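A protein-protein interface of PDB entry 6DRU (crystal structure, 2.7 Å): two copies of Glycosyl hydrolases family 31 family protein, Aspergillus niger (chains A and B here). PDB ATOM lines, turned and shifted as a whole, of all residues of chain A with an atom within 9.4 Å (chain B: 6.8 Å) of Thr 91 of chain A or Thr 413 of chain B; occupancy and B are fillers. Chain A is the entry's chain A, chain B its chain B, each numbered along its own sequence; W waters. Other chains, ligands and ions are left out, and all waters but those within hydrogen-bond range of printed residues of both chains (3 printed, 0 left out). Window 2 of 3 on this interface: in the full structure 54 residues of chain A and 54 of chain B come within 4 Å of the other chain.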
ATOM      1  N   HIS A  14      17.701   0.964  27.793  1.00  0.00           N
ATOM      2  CA  HIS A  14      17.532   0.113  26.618  1.00  0.00           C
ATOM      3  C   HIS A  14      16.379  -0.845  26.903  1.00  0.00           C
ATOM      4  O   HIS A  14      16.583  -1.957  27.389  1.00  0.00           O
ATOM      5  CB  HIS A  14      18.823  -0.635  26.307  1.00  0.00           C
ATOM      6  CG  HIS A  14      18.726  -1.542  25.122  1.00  0.00           C
ATOM      7  ND1 HIS A  14      19.159  -2.850  25.151  1.00  0.00           N
ATOM      8  CD2 HIS A  14      18.253  -1.329  23.870  1.00  0.00           C
ATOM      9  CE1 HIS A  14      18.955  -3.405  23.969  1.00  0.00           C
ATOM     10  NE2 HIS A  14      18.407  -2.503  23.174  1.00  0.00           N
ATOM     11  N   GLY A  70      19.686   5.246  24.136  1.00  0.00           N
ATOM     12  CA  GLY A  70      20.542   4.536  23.204  1.00  0.00           C
ATOM     13  C   GLY A  70      20.098   4.601  21.762  1.00  0.00           C
ATOM     14  O   GLY A  70      20.389   3.680  20.991  1.00  0.00           O
ATOM     15  N   THR A  71      19.395   5.665  21.372  1.00  0.00           N
ATOM     16  CA  THR A  71      18.960   5.806  19.987  1.00  0.00           C
ATOM     17  C   THR A  71      20.095   6.264  19.079  1.00  0.00           C
ATOM     18  O   THR A  71      20.087   5.953  17.882  1.00  0.00           O
ATOM     19  CB  THR A  71      17.787   6.784  19.893  1.00  0.00           C
ATOM     20  OG1 THR A  71      18.179   8.059  20.418  1.00  0.00           O
ATOM     21  CG2 THR A  71      16.597   6.261  20.680  1.00  0.00           C
ATOM     22  N   GLU A  72      21.064   6.993  19.623  1.00  0.00           N
ATOM     23  CA  GLU A  72      22.166   7.567  18.869  1.00  0.00           C
ATOM     24  C   GLU A  72      23.492   7.175  19.500  1.00  0.00           C
ATOM     25  O   GLU A  72      23.570   6.959  20.713  1.00  0.00           O
ATOM     26  CB  GLU A  72      22.057   9.099  18.818  1.00  0.00           C
ATOM     27  CG  GLU A  72      20.827   9.616  18.088  1.00  0.00           C
ATOM     28  CD  GLU A  72      20.869   9.323  16.601  1.00  0.00           C
ATOM     29  OE1 GLU A  72      21.769   9.855  15.916  1.00  0.00           O
ATOM     30  OE2 GLU A  72      20.005   8.562  16.115  1.00  0.00           O
ATOM     31  N   PRO A  73      24.548   7.056  18.696  1.00  0.00           N
ATOM     32  CA  PRO A  73      25.855   6.676  19.247  1.00  0.00           C
ATOM     33  C   PRO A  73      26.487   7.804  20.049  1.00  0.00           C
ATOM     34  O   PRO A  73      26.282   8.988  19.773  1.00  0.00           O
ATOM     35  CB  PRO A  73      26.684   6.352  17.999  1.00  0.00           C
ATOM     36  CG  PRO A  73      26.029   7.117  16.904  1.00  0.00           C
ATOM     37  CD  PRO A  73      24.566   7.126  17.226  1.00  0.00           C
ATOM     38  N   THR A  85      29.471   3.720  22.144  1.00  0.00           N
ATOM     39  CA  THR A  85      28.183   3.049  22.029  1.00  0.00           C
ATOM     40  C   THR A  85      27.759   3.022  20.566  1.00  0.00           C
ATOM     41  O   THR A  85      27.847   4.035  19.867  1.00  0.00           O
ATOM     42  CB  THR A  85      27.122   3.747  22.883  1.00  0.00           C
ATOM     43  OG1 THR A  85      26.930   5.091  22.421  1.00  0.00           O
ATOM     44  CG2 THR A  85      27.542   3.770  24.347  1.00  0.00           C
ATOM     45  N   THR A  86      27.314   1.857  20.100  1.00  0.00           N
ATOM     46  CA  THR A  86      26.960   1.663  18.702  1.00  0.00           C
ATOM     47  C   THR A  86      25.663   0.868  18.623  1.00  0.00           C
ATOM     48  O   THR A  86      25.102   0.447  19.640  1.00  0.00           O
ATOM     49  CB  THR A  86      28.078   0.950  17.931  1.00  0.00           C
ATOM     50  OG1 THR A  86      28.440  -0.258  18.614  1.00  0.00           O
ATOM     51  CG2 THR A  86      29.302   1.849  17.795  1.00  0.00           C
ATOM     52  N   GLY A  87      25.185   0.670  17.395  1.00  0.00           N
ATOM     53  CA  GLY A  87      24.029  -0.161  17.141  1.00  0.00           C
ATOM     54  C   GLY A  87      24.416  -1.609  16.908  1.00  0.00           C
ATOM     55  O   GLY A  87      25.557  -2.026  17.119  1.00  0.00           O
ATOM     56  N   TRP A  88      23.434  -2.389  16.467  1.00  0.00           N
ATOM     57  CA  TRP A  88      23.625  -3.798  16.151  1.00  0.00           C
ATOM     58  C   TRP A  88      23.236  -4.038  14.700  1.00  0.00           C
ATOM     59  O   TRP A  88      22.163  -3.614  14.261  1.00  0.00           O
ATOM     60  CB  TRP A  88      22.806  -4.692  17.086  1.00  0.00           C
ATOM     61  CG  TRP A  88      22.318  -5.945  16.437  1.00  0.00           C
ATOM     62  CD1 TRP A  88      23.069  -7.017  16.047  1.00  0.00           C
ATOM     63  CD2 TRP A  88      20.963  -6.265  16.108  1.00  0.00           C
ATOM     64  NE1 TRP A  88      22.265  -7.981  15.489  1.00  0.00           N
ATOM     65  CE2 TRP A  88      20.967  -7.544  15.517  1.00  0.00           C
ATOM     66  CE3 TRP A  88      19.746  -5.594  16.256  1.00  0.00           C
ATOM     67  CZ2 TRP A  88      19.802  -8.163  15.074  1.00  0.00           C
ATOM     68  CZ3 TRP A  88      18.593  -6.210  15.816  1.00  0.00           C
ATOM     69  CH2 TRP A  88      18.627  -7.481  15.232  1.00  0.00           C
ATOM     70  N   GLY A  89      24.110  -4.717  13.962  1.00  0.00           N
ATOM     71  CA  GLY A  89      23.943  -4.808  12.526  1.00  0.00           C
ATOM     72  C   GLY A  89      24.375  -3.516  11.850  1.00  0.00           C
ATOM     73  O   GLY A  89      25.269  -2.807  12.318  1.00  0.00           O
ATOM     74  N   GLY A  90      23.720  -3.206  10.736  1.00  0.00           N
ATOM     75  CA  GLY A  90      24.001  -1.956  10.070  1.00  0.00           C
ATOM     76  C   GLY A  90      23.363  -0.735  10.688  1.00  0.00           C
ATOM     77  O   GLY A  90      23.463   0.358  10.127  1.00  0.00           O
ATOM     78  N   THR A  91      22.709  -0.890  11.836  1.00  0.00           N
ATOM     79  CA  THR A  91      21.987   0.213  12.452  1.00  0.00           C
ATOM     80  C   THR A  91      22.946   1.205  13.102  1.00  0.00           C
ATOM     81  O   THR A  91      24.065   0.862  13.492  1.00  0.00           O
ATOM     82  CB  THR A  91      20.997  -0.313  13.491  1.00  0.00           C
ATOM     83  OG1 THR A  91      21.644  -1.280  14.326  1.00  0.00           O
ATOM     84  CG2 THR A  91      19.810  -0.964  12.803  1.00  0.00           C
ATOM     85  N   THR A  92      22.485   2.446  13.225  1.00  0.00           N
ATOM     86  CA  THR A  92      23.205   3.507  13.924  1.00  0.00           C
ATOM     87  C   THR A  92      22.448   3.822  15.209  1.00  0.00           C
ATOM     88  O   THR A  92      21.423   4.508  15.184  1.00  0.00           O
ATOM     89  CB  THR A  92      23.338   4.745  13.044  1.00  0.00           C
ATOM     90  OG1 THR A  92      24.006   4.392  11.826  1.00  0.00           O
ATOM     91  CG2 THR A  92      24.135   5.822  13.763  1.00  0.00           C
ATOM     92  N   ALA A  93      22.956   3.319  16.330  1.00  0.00           N
ATOM     93  CA  ALA A  93      22.305   3.508  17.620  1.00  0.00           C
ATOM     94  C   ALA A  93      23.380   3.561  18.701  1.00  0.00           C
ATOM     95  O   ALA A  93      24.565   3.743  18.412  1.00  0.00           O
ATOM     96  CB  ALA A  93      21.275   2.399  17.862  1.00  0.00           C
ATOM     97  N   GLY A  94      22.961   3.417  19.957  1.00  0.00           N
ATOM     98  CA  GLY A  94      23.892   3.490  21.066  1.00  0.00           C
ATOM     99  C   GLY A  94      23.534   2.622  22.257  1.00  0.00           C
ATOM    100  O   GLY A  94      23.586   3.084  23.400  1.00  0.00           O
ATOM    101  N   TYR A  95      23.172   1.363  22.007  1.00  0.00           N
ATOM    102  CA  TYR A  95      22.872   0.412  23.069  1.00  0.00           C
ATOM    103  C   TYR A  95      23.852  -0.751  23.124  1.00  0.00           C
ATOM    104  O   TYR A  95      23.674  -1.657  23.946  1.00  0.00           O
ATOM    105  CB  TYR A  95      21.440  -0.123  22.918  1.00  0.00           C
ATOM    106  CG  TYR A  95      21.125  -0.653  21.538  1.00  0.00           C
ATOM    107  CD1 TYR A  95      21.579  -1.902  21.130  1.00  0.00           C
ATOM    108  CD2 TYR A  95      20.370   0.091  20.644  1.00  0.00           C
ATOM    109  CE1 TYR A  95      21.298  -2.386  19.867  1.00  0.00           C
ATOM    110  CE2 TYR A  95      20.077  -0.390  19.381  1.00  0.00           C
ATOM    111  CZ  TYR A  95      20.545  -1.626  18.996  1.00  0.00           C
ATOM    112  OH  TYR A  95      20.257  -2.103  17.736  1.00  0.00           O
ATOM    113  N   ARG A  96      24.874  -0.756  22.272  1.00  0.00           N
ATOM    114  CA  ARG A  96      25.923  -1.764  22.291  1.00  0.00           C
ATOM    115  C   ARG A  96      27.242  -1.110  22.678  1.00  0.00           C
ATOM    116  O   ARG A  96      27.522   0.022  22.274  1.00  0.00           O
ATOM    117  CB  ARG A  96      26.050  -2.453  20.929  1.00  0.00           C
ATOM    118  CG  ARG A  96      24.871  -3.343  20.585  1.00  0.00           C
ATOM    119  CD  ARG A  96      24.998  -4.710  21.243  1.00  0.00           C
ATOM    120  NE  ARG A  96      23.741  -5.451  21.200  1.00  0.00           N
ATOM    121  CZ  ARG A  96      22.868  -5.498  22.202  1.00  0.00           C
ATOM    122  NH1 ARG A  96      23.118  -4.852  23.332  1.00  0.00           N
ATOM    123  NH2 ARG A  96      21.748  -6.195  22.077  1.00  0.00           N
ATOM    124  N   ALA A 116      28.008  -9.207  19.222  1.00  0.00           N
ATOM    125  CA  ALA A 116      26.709  -9.060  18.562  1.00  0.00           C
ATOM    126  C   ALA A 116      26.897  -8.955  17.055  1.00  0.00           C
ATOM    127  O   ALA A 116      26.696  -7.893  16.455  1.00  0.00           O
ATOM    128  CB  ALA A 116      25.960  -7.842  19.107  1.00  0.00           C
ATOM    129  N   LEU A 118      25.433 -10.155  13.210  1.00  0.00           N
ATOM    130  CA  LEU A 118      24.059 -10.047  12.726  1.00  0.00           C
ATOM    131  C   LEU A 118      23.179 -11.143  13.312  1.00  0.00           C
ATOM    132  O   LEU A 118      22.103 -10.869  13.855  1.00  0.00           O
ATOM    133  CB  LEU A 118      24.034 -10.099  11.200  1.00  0.00           C
ATOM    134  CG  LEU A 118      22.692  -9.743  10.563  1.00  0.00           C
ATOM    135  CD1 LEU A 118      22.341  -8.299  10.874  1.00  0.00           C
ATOM    136  CD2 LEU A 118      22.719  -9.984   9.063  1.00  0.00           C
ATOM    137  N   ASN A 122      21.580 -12.309  22.258  1.00  0.00           N
ATOM    138  CA  ASN A 122      21.791 -10.988  22.827  1.00  0.00           C
ATOM    139  C   ASN A 122      23.027 -11.005  23.720  1.00  0.00           C
ATOM    140  O   ASN A 122      23.144 -11.876  24.593  1.00  0.00           O
ATOM    141  CB  ASN A 122      20.566 -10.542  23.622  1.00  0.00           C
ATOM    142  CG  ASN A 122      20.543  -9.046  23.858  1.00  0.00           C
ATOM    143  OD1 ASN A 122      21.287  -8.529  24.691  1.00  0.00           O
ATOM    144  ND2 ASN A 122      19.692  -8.341  23.121  1.00  0.00           N
ATOM    145  N   GLN B 411       9.508  -6.285  14.067  1.00  0.00           N
ATOM    146  CA  GLN B 411       9.409  -4.950  14.635  1.00  0.00           C
ATOM    147  C   GLN B 411      10.733  -4.214  14.430  1.00  0.00           C
ATOM    148  O   GLN B 411      11.638  -4.699  13.746  1.00  0.00           O
ATOM    149  CB  GLN B 411       9.017  -5.032  16.107  1.00  0.00           C
ATOM    150  CG  GLN B 411       7.660  -5.663  16.340  1.00  0.00           C
ATOM    151  CD  GLN B 411       7.246  -5.632  17.795  1.00  0.00           C
ATOM    152  OE1 GLN B 411       6.986  -6.672  18.402  1.00  0.00           O
ATOM    153  NE2 GLN B 411       7.180  -4.433  18.366  1.00  0.00           N
ATOM    154  N   SER B 412      10.856  -3.031  15.026  1.00  0.00           N
ATOM    155  CA  SER B 412      12.058  -2.228  14.858  1.00  0.00           C
ATOM    156  C   SER B 412      13.280  -2.962  15.398  1.00  0.00           C
ATOM    157  O   SER B 412      13.180  -3.819  16.279  1.00  0.00           O
ATOM    158  CB  SER B 412      11.902  -0.882  15.567  1.00  0.00           C
ATOM    159  OG  SER B 412      11.913  -1.046  16.975  1.00  0.00           O
ATOM    160  N   THR B 413      14.450  -2.619  14.853  1.00  0.00           N
ATOM    161  CA  THR B 413      15.686  -3.243  15.312  1.00  0.00           C
ATOM    162  C   THR B 413      16.009  -2.859  16.748  1.00  0.00           C
ATOM    163  O   THR B 413      16.673  -3.625  17.457  1.00  0.00           O
ATOM    164  CB  THR B 413      16.843  -2.862  14.392  1.00  0.00           C
ATOM    165  OG1 THR B 413      17.141  -1.470  14.553  1.00  0.00           O
ATOM    166  CG2 THR B 413      16.478  -3.131  12.941  1.00  0.00           C
ATOM    167  N   TYR B 414      15.549  -1.690  17.198  1.00  0.00           N
ATOM    168  CA  TYR B 414      15.726  -1.316  18.597  1.00  0.00           C
ATOM    169  C   TYR B 414      14.948  -2.254  19.512  1.00  0.00           C
ATOM    170  O   TYR B 414      15.481  -2.750  20.511  1.00  0.00           O
ATOM    171  CB  TYR B 414      15.290   0.135  18.813  1.00  0.00           C
ATOM    172  CG  TYR B 414      15.532   0.652  20.216  1.00  0.00           C
ATOM    173  CD1 TYR B 414      14.594   0.454  21.225  1.00  0.00           C
ATOM    174  CD2 TYR B 414      16.697   1.339  20.532  1.00  0.00           C
ATOM    175  CE1 TYR B 414      14.814   0.923  22.507  1.00  0.00           C
ATOM    176  CE2 TYR B 414      16.923   1.812  21.809  1.00  0.00           C
ATOM    177  CZ  TYR B 414      15.978   1.601  22.793  1.00  0.00           C
ATOM    178  OH  TYR B 414      16.198   2.070  24.068  1.00  0.00           O
ATOM    179  N   ILE B 415      13.677  -2.503  19.186  1.00  0.00           N
ATOM    180  CA  ILE B 415      12.871  -3.426  19.983  1.00  0.00           C
ATOM    181  C   ILE B 415      13.440  -4.837  19.896  1.00  0.00           C
ATOM    182  O   ILE B 415      13.504  -5.560  20.898  1.00  0.00           O
ATOM    183  CB  ILE B 415      11.399  -3.375  19.535  1.00  0.00           C
ATOM    184  CG1 ILE B 415      10.780  -2.025  19.899  1.00  0.00           C
ATOM    185  CG2 ILE B 415      10.604  -4.514  20.152  1.00  0.00           C
ATOM    186  CD1 ILE B 415       9.387  -1.835  19.360  1.00  0.00           C
ATOM    187  N   GLU B 416      13.860  -5.251  18.697  1.00  0.00           N
ATOM    188  CA  GLU B 416      14.469  -6.566  18.535  1.00  0.00           C
ATOM    189  C   GLU B 416      15.721  -6.712  19.389  1.00  0.00           C
ATOM    190  O   GLU B 416      16.038  -7.818  19.840  1.00  0.00           O
ATOM    191  CB  GLU B 416      14.802  -6.811  17.063  1.00  0.00           C
ATOM    192  CG  GLU B 416      13.593  -7.066  16.175  1.00  0.00           C
ATOM    193  CD  GLU B 416      13.946  -7.066  14.698  1.00  0.00           C
ATOM    194  OE1 GLU B 416      15.018  -6.531  14.345  1.00  0.00           O
ATOM    195  OE2 GLU B 416      13.156  -7.603  13.891  1.00  0.00           O
ATOM    196  N   SER B 417      16.443  -5.614  19.622  1.00  0.00           N
ATOM    197  CA  SER B 417      17.661  -5.664  20.419  1.00  0.00           C
ATOM    198  C   SER B 417      17.391  -5.691  21.917  1.00  0.00           C
ATOM    199  O   SER B 417      18.295  -6.034  22.686  1.00  0.00           O
ATOM    200  CB  SER B 417      18.555  -4.469  20.088  1.00  0.00           C
ATOM    201  OG  SER B 417      17.937  -3.251  20.467  1.00  0.00           O
ATOM    202  N   ILE B 418      16.181  -5.342  22.344  1.00  0.00           N
ATOM    203  CA  ILE B 418      15.850  -5.420  23.771  1.00  0.00           C
ATOM    204  C   ILE B 418      15.894  -6.878  24.210  1.00  0.00           C
ATOM    205  O   ILE B 418      15.259  -7.739  23.568  1.00  0.00           O
ATOM    206  CB  ILE B 418      14.469  -4.798  24.040  1.00  0.00           C
ATOM    207  CG1 ILE B 418      14.434  -3.355  23.537  1.00  0.00           C
ATOM    208  CG2 ILE B 418      14.131  -4.851  25.522  1.00  0.00           C
ATOM    209  CD1 ILE B 418      13.071  -2.707  23.622  1.00  0.00           C
ATOM    210  N   SER B 524      24.280  -2.555   5.071  1.00  0.00           N
ATOM    211  CA  SER B 524      24.022  -1.121   5.017  1.00  0.00           C
ATOM    212  C   SER B 524      25.299  -0.295   5.094  1.00  0.00           C
ATOM    213  O   SER B 524      25.294   0.868   4.674  1.00  0.00           O
ATOM    214  CB  SER B 524      23.068  -0.715   6.140  1.00  0.00           C
ATOM    215  OG  SER B 524      23.773  -0.482   7.344  1.00  0.00           O
ATOM    216  N   THR B 525      26.387  -0.859   5.619  1.00  0.00           N
ATOM    217  CA  THR B 525      27.646  -0.130   5.712  1.00  0.00           C
ATOM    218  C   THR B 525      28.462  -0.197   4.428  1.00  0.00           C
ATOM    219  O   THR B 525      29.432   0.556   4.292  1.00  0.00           O
ATOM    220  CB  THR B 525      28.481  -0.669   6.875  1.00  0.00           C
ATOM    221  OG1 THR B 525      28.820  -2.039   6.625  1.00  0.00           O
ATOM    222  CG2 THR B 525      27.696  -0.580   8.172  1.00  0.00           C
HETATM  223  O   HOH W   1      20.667  -5.961  25.011  1.00  0.00           O
HETATM  224  O   HOH W   2      18.983  -0.109  16.029  1.00  0.00           O
HETATM  225  O   HOH W   3      17.345  -9.657  21.638  1.00  0.00           O
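A ring nitrogen (NE2) of His 14 of chain A lies within hydrogen-bond range of the side-chain hydroxyl of Ser 417 of chain B (2.8 Å). The side-chain hydroxyl (OG) of Ser 524 of chain B is in hydrogen-bond range of the backbone carbonyl oxygen (O) of Gly 90 of chain A (2.9 Å). The side-chain amide nitrogen (ND2) of Asn 122 of chain A sits at hydrogen-bond distance from the backbone carbonyl oxygen (O) of Ser 417 of chain B.
The backbone NH (N) of Tyr 95 of chain A sits at hydrogen-bond distance from the backbone carbonyl oxygen (O) of Thr 86 of chain A. N of Thr 86 of chain A is in hydrogen-bond range of O of Arg 96 of chain A (2.9 Å). The backbone NH of Trp 88 of chain A is in hydrogen-bond range of the side-chain hydroxyl of Thr 91 of chain A (3.0 Å). The backbone NH (N) of Trp 88 of chain A sits at hydrogen-bond distance from the side-chain hydroxyl (OH) of Tyr 95 of chain A (3.4 Å). O of Thr 413 of chain B is in hydrogen-bond range of OG of Ser 417 of chain B, at 3.3 Å. The backbone carbonyl oxygen (O) of Tyr 414 of chain B is in hydrogen-bond range of the side-chain hydroxyl (OG) of Ser 417 of chain B (2.5 Å).
Tyr 414 of chain B touches His 14 of chain A (OH to CA, 3.5 Å). NE2 of His 14 of chain A touches N of Ile 418 of chain B (3.7 Å). CZ3 of Trp 88 of chain A touches O of Thr 413 of chain B, 3.6 Å away. Glu 416 of chain B touches Trp 88 of chain A (OE1 to CH2, 3.8 Å). Thr 413 of chain B touches Thr 91 of chain A. OH of Tyr 95 of chain A touches O of Thr 413 of chain B, at 3.9 Å. CD2 of Tyr 414 of chain B touches CD2 of Tyr 95 of chain A (3.9 Å). CZ of Tyr 95 of chain A touches OG of Ser 417 of chain B, 3.4 Å away. Arg 96 of chain A touches Ser 417 of chain B (NH2 to O, 3.5 Å).
Thr 91 of chain A touches one residue of chain B. Of chain A, only Trp 88, Thr 91 and Tyr 95 come within 4 Å of Thr 413 of chain B. No residue of chain A comes within 4 Å of Ser 412 of chain B. Glu 416 of chain B touches just one residue of chain A: Trp 88 (3.8 Å). Of the printed residues of chain A, Ile 418 of chain B touches His 14. Of the printed residues of chain B, Asn 122 of chain A touches Ser 417. Printed residues of chain B within 4 Å of Tyr 95 of chain A: Thr 413, Tyr 414 and Ser 417. Printed residues of chain A within 4 Å of Tyr 414 of chain B: His 14 and Tyr 95. Ile 415 of chain B touches none of the printed residues of chain A. Gly 89 of chain A touches none of the printed residues of chain B. The nearest residue of chain B that does not touch Thr 91 of chain A is Ser 524 of chain B (4.6 Å). The nearest residue of chain A that does not touch Thr 413 of chain B is His 14 of chain A (6.1 Å).
Of the 20 printed residues of chain A, 7 touch a printed residue of chain B. Hydrophobic or aromatic side chains of chain A within 4 Å of the printed part of chain B: His 14, Trp 88 and Tyr 95. Along chain A the printed residues that touch a printed residue of chain B span positions 14 to 122. Of the 10 printed residues of chain B, 6 touch a printed residue of chain A. Among the printed residues, no Asp or Glu carboxylate lies within 4 Å of a Lys or Arg side-chain nitrogen of the other chain.
No position is printed for both chains. Of the 12 pairs that touch across the chains among the printed residues, none has its exchanged pair printed and touching as well.
Water W1 lies within hydrogen-bond range of OD1 of Asn 122 of chain A (2.7 Å), NH2 of Arg 96 of chain A (3.1 Å), O of Ser 417 of chain B (3.3 Å) and ND1 of His 14 of chain A (3.5 Å). Water W2 lies within hydrogen-bond range of the side-chain hydroxyl (OG1) of Thr 413 of chain B, the side-chain hydroxyl (OH) of Tyr 95 of chain A and the side-chain hydroxyl (OG1) of Thr 91 of chain A. Water W3 lies within hydrogen-bond range of the backbone carbonyl oxygen (O) of Glu 416 of chain B (2.9 Å), the side-chain amide nitrogen (ND2) of Asn 122 of chain A (3.1 Å) and the backbone carbonyl oxygen (O) of Ile 418 of chain B (3.4 Å).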
